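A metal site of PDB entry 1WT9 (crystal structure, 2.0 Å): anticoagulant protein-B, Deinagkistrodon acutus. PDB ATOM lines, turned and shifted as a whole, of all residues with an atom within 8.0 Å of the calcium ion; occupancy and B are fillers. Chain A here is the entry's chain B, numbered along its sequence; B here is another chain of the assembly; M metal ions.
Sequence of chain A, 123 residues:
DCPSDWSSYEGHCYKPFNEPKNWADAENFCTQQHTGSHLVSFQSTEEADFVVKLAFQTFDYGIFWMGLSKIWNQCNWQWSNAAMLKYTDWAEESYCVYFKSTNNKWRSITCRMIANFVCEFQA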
ATOM      1  N   TYR A   9      31.628  -7.010  28.055  1.00  0.00           N
ATOM      2  CA  TYR A   9      32.028  -7.657  26.810  1.00  0.00           C
ATOM      3  C   TYR A   9      31.715  -6.708  25.662  1.00  0.00           C
ATOM      4  O   TYR A   9      30.572  -6.305  25.478  1.00  0.00           O
ATOM      5  CB  TYR A   9      31.284  -8.966  26.607  1.00  0.00           C
ATOM      6  CG  TYR A   9      31.493  -9.527  25.220  1.00  0.00           C
ATOM      7  CD1 TYR A   9      32.730 -10.034  24.843  1.00  0.00           C
ATOM      8  CD2 TYR A   9      30.486  -9.453  24.256  1.00  0.00           C
ATOM      9  CE1 TYR A   9      32.967 -10.469  23.544  1.00  0.00           C
ATOM     10  CE2 TYR A   9      30.713  -9.885  22.958  1.00  0.00           C
ATOM     11  CZ  TYR A   9      31.947 -10.383  22.604  1.00  0.00           C
ATOM     12  OH  TYR A   9      32.186 -10.789  21.321  1.00  0.00           O
ATOM     13  N   HIS A  12      29.550  -3.731  26.253  1.00  0.00           N
ATOM     14  CA  HIS A  12      28.207  -4.009  26.752  1.00  0.00           C
ATOM     15  C   HIS A  12      28.316  -4.670  28.115  1.00  0.00           C
ATOM     16  O   HIS A  12      29.357  -5.216  28.468  1.00  0.00           O
ATOM     17  CB  HIS A  12      27.452  -4.925  25.787  1.00  0.00           C
ATOM     18  CG  HIS A  12      26.812  -4.216  24.648  1.00  0.00           C
ATOM     19  ND1 HIS A  12      27.450  -3.229  23.912  1.00  0.00           N
ATOM     20  CD2 HIS A  12      25.591  -4.357  24.077  1.00  0.00           C
ATOM     21  CE1 HIS A  12      26.650  -2.807  22.959  1.00  0.00           C
ATOM     22  NE2 HIS A  12      25.521  -3.475  23.027  1.00  0.00           N
ATOM     23  N   TYR A  14      26.448  -7.463  30.769  1.00  0.00           N
ATOM     24  CA  TYR A  14      25.530  -8.591  30.849  1.00  0.00           C
ATOM     25  C   TYR A  14      25.391  -9.130  32.269  1.00  0.00           C
ATOM     26  O   TYR A  14      26.334  -9.071  33.057  1.00  0.00           O
ATOM     27  CB  TYR A  14      26.032  -9.726  29.943  1.00  0.00           C
ATOM     28  CG  TYR A  14      26.317  -9.319  28.513  1.00  0.00           C
ATOM     29  CD1 TYR A  14      27.433  -8.552  28.200  1.00  0.00           C
ATOM     30  CD2 TYR A  14      25.455  -9.692  27.479  1.00  0.00           C
ATOM     31  CE1 TYR A  14      27.689  -8.165  26.875  1.00  0.00           C
ATOM     32  CE2 TYR A  14      25.701  -9.308  26.163  1.00  0.00           C
ATOM     33  CZ  TYR A  14      26.815  -8.555  25.864  1.00  0.00           C
ATOM     34  OH  TYR A  14      27.052  -8.176  24.571  1.00  0.00           O
ATOM     35  N   LEU A  39      16.359  -7.822  27.735  1.00  0.00           N
ATOM     36  CA  LEU A  39      16.754  -9.227  27.653  1.00  0.00           C
ATOM     37  C   LEU A  39      17.883  -9.217  26.624  1.00  0.00           C
ATOM     38  O   LEU A  39      17.872  -8.414  25.690  1.00  0.00           O
ATOM     39  CB  LEU A  39      15.592 -10.090  27.164  1.00  0.00           C
ATOM     40  CG  LEU A  39      14.606 -10.553  28.231  1.00  0.00           C
ATOM     41  CD1 LEU A  39      13.430 -11.233  27.567  1.00  0.00           C
ATOM     42  CD2 LEU A  39      15.304 -11.500  29.197  1.00  0.00           C
ATOM     43  N   VAL A  40      18.873 -10.091  26.796  1.00  0.00           N
ATOM     44  CA  VAL A  40      19.998 -10.123  25.881  1.00  0.00           C
ATOM     45  C   VAL A  40      19.634 -10.296  24.398  1.00  0.00           C
ATOM     46  O   VAL A  40      18.640 -10.938  24.056  1.00  0.00           O
ATOM     47  CB  VAL A  40      21.005 -11.240  26.297  1.00  0.00           C
ATOM     48  CG1 VAL A  40      20.387 -12.615  26.090  1.00  0.00           C
ATOM     49  CG2 VAL A  40      22.284 -11.092  25.529  1.00  0.00           C
ATOM     50  N   SER A  41      20.434  -9.679  23.543  1.00  0.00           N
ATOM     51  CA  SER A  41      20.266  -9.768  22.088  1.00  0.00           C
ATOM     52  C   SER A  41      21.594 -10.248  21.524  1.00  0.00           C
ATOM     53  O   SER A  41      22.657  -9.874  22.034  1.00  0.00           O
ATOM     54  CB  SER A  41      19.898  -8.407  21.488  1.00  0.00           C
ATOM     55  OG  SER A  41      20.897  -7.446  21.737  1.00  0.00           O
ATOM     56  N   PHE A  42      21.564 -11.075  20.488  1.00  0.00           N
ATOM     57  CA  PHE A  42      22.797 -11.605  19.903  1.00  0.00           C
ATOM     58  C   PHE A  42      23.056 -11.100  18.497  1.00  0.00           C
ATOM     59  O   PHE A  42      22.297 -11.386  17.565  1.00  0.00           O
ATOM     60  CB  PHE A  42      22.746 -13.127  19.892  1.00  0.00           C
ATOM     61  CG  PHE A  42      22.764 -13.742  21.259  1.00  0.00           C
ATOM     62  CD1 PHE A  42      22.133 -14.966  21.500  1.00  0.00           C
ATOM     63  CD2 PHE A  42      23.424 -13.121  22.311  1.00  0.00           C
ATOM     64  CE1 PHE A  42      22.172 -15.552  22.757  1.00  0.00           C
ATOM     65  CE2 PHE A  42      23.467 -13.701  23.575  1.00  0.00           C
ATOM     66  CZ  PHE A  42      22.834 -14.918  23.795  1.00  0.00           C
ATOM     67  N   GLN A  43      24.135 -10.341  18.341  1.00  0.00           N
ATOM     68  CA  GLN A  43      24.526  -9.797  17.051  1.00  0.00           C
ATOM     69  C   GLN A  43      25.657 -10.591  16.412  1.00  0.00           C
ATOM     70  O   GLN A  43      26.021 -10.336  15.270  1.00  0.00           O
ATOM     71  CB  GLN A  43      24.968  -8.333  17.192  1.00  0.00           C
ATOM     72  CG  GLN A  43      23.865  -7.301  16.990  1.00  0.00           C
ATOM     73  CD  GLN A  43      22.787  -7.366  18.043  1.00  0.00           C
ATOM     74  OE1 GLN A  43      23.066  -7.377  19.245  1.00  0.00           O
ATOM     75  NE2 GLN A  43      21.528  -7.381  17.607  1.00  0.00           N
ATOM     76  N   SER A  44      26.209 -11.551  17.144  1.00  0.00           N
ATOM     77  CA  SER A  44      27.302 -12.361  16.612  1.00  0.00           C
ATOM     78  C   SER A  44      27.509 -13.642  17.409  1.00  0.00           C
ATOM     79  O   SER A  44      26.933 -13.826  18.491  1.00  0.00           O
ATOM     80  CB  SER A  44      28.601 -11.548  16.615  1.00  0.00           C
ATOM     81  OG  SER A  44      29.080 -11.357  17.936  1.00  0.00           O
ATOM     82  N   GLU A  47      29.595 -13.070  20.784  1.00  0.00           N
ATOM     83  CA  GLU A  47      28.767 -12.548  21.867  1.00  0.00           C
ATOM     84  C   GLU A  47      27.945 -13.682  22.469  1.00  0.00           C
ATOM     85  O   GLU A  47      27.815 -13.799  23.686  1.00  0.00           O
ATOM     86  CB  GLU A  47      27.846 -11.439  21.357  1.00  0.00           C
ATOM     87  CG  GLU A  47      26.784 -11.024  22.367  1.00  0.00           C
ATOM     88  CD  GLU A  47      25.936  -9.849  21.891  1.00  0.00           C
ATOM     89  OE1 GLU A  47      25.742  -9.704  20.668  1.00  0.00           O
ATOM     90  OE2 GLU A  47      25.454  -9.066  22.747  1.00  0.00           O
ATOM     91  N   ALA A  48      27.403 -14.528  21.593  1.00  0.00           N
ATOM     92  CA  ALA A  48      26.602 -15.664  22.026  1.00  0.00           C
ATOM     93  C   ALA A  48      27.402 -16.616  22.917  1.00  0.00           C
ATOM     94  O   ALA A  48      26.923 -17.012  23.986  1.00  0.00           O
ATOM     95  CB  ALA A  48      26.071 -16.411  20.808  1.00  0.00           C
ATOM     96  N   VAL A  51      28.020 -14.967  26.465  1.00  0.00           N
ATOM     97  CA  VAL A  51      26.839 -15.028  27.306  1.00  0.00           C
ATOM     98  C   VAL A  51      26.510 -16.444  27.787  1.00  0.00           C
ATOM     99  O   VAL A  51      26.082 -16.640  28.936  1.00  0.00           O
ATOM    100  CB  VAL A  51      25.628 -14.443  26.554  1.00  0.00           C
ATOM    101  CG1 VAL A  51      24.372 -14.545  27.413  1.00  0.00           C
ATOM    102  CG2 VAL A  51      25.903 -13.000  26.192  1.00  0.00           C
ATOM    103  N   GLU A 120      20.982  -7.195  29.445  1.00  0.00           N
ATOM    104  CA  GLU A 120      22.098  -6.542  28.775  1.00  0.00           C
ATOM    105  C   GLU A 120      21.833  -5.065  28.508  1.00  0.00           C
ATOM    106  O   GLU A 120      20.699  -4.665  28.265  1.00  0.00           O
ATOM    107  CB  GLU A 120      22.385  -7.249  27.439  1.00  0.00           C
ATOM    108  CG  GLU A 120      23.054  -6.365  26.376  1.00  0.00           C
ATOM    109  CD  GLU A 120      23.281  -7.096  25.049  1.00  0.00           C
ATOM    110  OE1 GLU A 120      22.429  -7.929  24.666  1.00  0.00           O
ATOM    111  OE2 GLU A 120      24.289  -6.817  24.371  1.00  0.00           O
ATOM    112  N   PHE A 121      22.891  -4.259  28.552  1.00  0.00           N
ATOM    113  CA  PHE A 121      22.780  -2.849  28.255  1.00  0.00           C
ATOM    114  C   PHE A 121      24.088  -2.321  27.689  1.00  0.00           C
ATOM    115  O   PHE A 121      25.144  -2.918  27.878  1.00  0.00           O
ATOM    116  CB  PHE A 121      22.323  -2.048  29.489  1.00  0.00           C
ATOM    117  CG  PHE A 121      23.357  -1.921  30.573  1.00  0.00           C
ATOM    118  CD1 PHE A 121      24.373  -0.968  30.474  1.00  0.00           C
ATOM    119  CD2 PHE A 121      23.273  -2.712  31.719  1.00  0.00           C
ATOM    120  CE1 PHE A 121      25.292  -0.810  31.516  1.00  0.00           C
ATOM    121  CE2 PHE A 121      24.201  -2.557  32.759  1.00  0.00           C
ATOM    122  CZ  PHE A 121      25.209  -1.594  32.654  1.00  0.00           C
ATOM    123  N   TRP B  83      14.608  -7.149  18.021  1.00  0.00           N
ATOM    124  CA  TRP B  83      14.801  -7.681  19.369  1.00  0.00           C
ATOM    125  C   TRP B  83      14.100  -6.725  20.336  1.00  0.00           C
ATOM    126  O   TRP B  83      13.713  -5.625  19.942  1.00  0.00           O
ATOM    127  CB  TRP B  83      16.280  -7.704  19.729  1.00  0.00           C
ATOM    128  CG  TRP B  83      17.120  -8.625  18.919  1.00  0.00           C
ATOM    129  CD1 TRP B  83      17.682  -8.371  17.692  1.00  0.00           C
ATOM    130  CD2 TRP B  83      17.521  -9.946  19.278  1.00  0.00           C
ATOM    131  NE1 TRP B  83      18.425  -9.457  17.285  1.00  0.00           N
ATOM    132  CE2 TRP B  83      18.334 -10.441  18.235  1.00  0.00           C
ATOM    133  CE3 TRP B  83      17.270 -10.763  20.386  1.00  0.00           C
ATOM    134  CZ2 TRP B  83      18.905 -11.711  18.273  1.00  0.00           C
ATOM    135  CZ3 TRP B  83      17.832 -12.030  20.426  1.00  0.00           C
ATOM    136  CH2 TRP B  83      18.646 -12.488  19.378  1.00  0.00           C
ATOM    137  N   ASP B  85      15.372  -4.982  22.468  1.00  0.00           N
ATOM    138  CA  ASP B  85      16.190  -3.780  22.631  1.00  0.00           C
ATOM    139  C   ASP B  85      16.183  -2.869  21.407  1.00  0.00           C
ATOM    140  O   ASP B  85      16.958  -1.916  21.343  1.00  0.00           O
ATOM    141  CB  ASP B  85      17.638  -4.121  23.010  1.00  0.00           C
ATOM    142  CG  ASP B  85      18.398  -4.815  21.873  1.00  0.00           C
ATOM    143  OD1 ASP B  85      17.935  -4.801  20.718  1.00  0.00           O
ATOM    144  OD2 ASP B  85      19.484  -5.377  22.159  1.00  0.00           O
ATOM    145  N   SER B  87      17.230  -3.326  18.314  1.00  0.00           N
ATOM    146  CA  SER B  87      18.145  -3.654  17.226  1.00  0.00           C
ATOM    147  C   SER B  87      17.537  -4.613  16.212  1.00  0.00           C
ATOM    148  O   SER B  87      16.649  -5.414  16.541  1.00  0.00           O
ATOM    149  CB  SER B  87      19.433  -4.253  17.791  1.00  0.00           C
ATOM    150  OG  SER B  87      19.171  -5.412  18.554  1.00  0.00           O
HETATM  151 CA    CA M   1      23.586  -7.703  22.048  1.00  0.00          CA
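Within 4 Å of the calcium ion: Ser 41, Gln 43, Glu 47 and Glu 120.
The nearest printed residue that does not touch the calcium ion is Phe 42 (4.2 Å).
The side-chain hydroxyl (OH) of Tyr 9 sits at hydrogen-bond distance from the backbone NH (N) of Glu 47, at 3.5 Å.
The side-chain amide nitrogen (NE2) of Gln 43 lies within hydrogen-bond range of the side-chain hydroxyl (OG) of Ser 87 of chain B, at 3.2 Å.
The side-chain hydroxyl (OH) of Tyr 14 lies close to the side-chain carboxylate (OE2) of Glu 47.
OG of Ser 44 is in hydrogen-bond range of N of Glu 47, at 3.4 Å.
The side-chain hydroxyl (OH) of Tyr 14 lies close to the side-chain carboxylate (OE2) of Glu 120.
OG of Ser 41 lies close to OD2 of Asp 85 of chain B (2.5 Å).
The calcium ion is bound by O of Ser 41 (2.4 Å), OE2 of Glu 47 (2.4 Å), OE2 of Glu 120 (2.6 Å), OG of Ser 41 (2.7 Å), OE1 of Gln 43 (2.9 Å) and OE1 of Glu 120 (2.9 Å).
The calcium ion has six donor atoms within binding distance.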
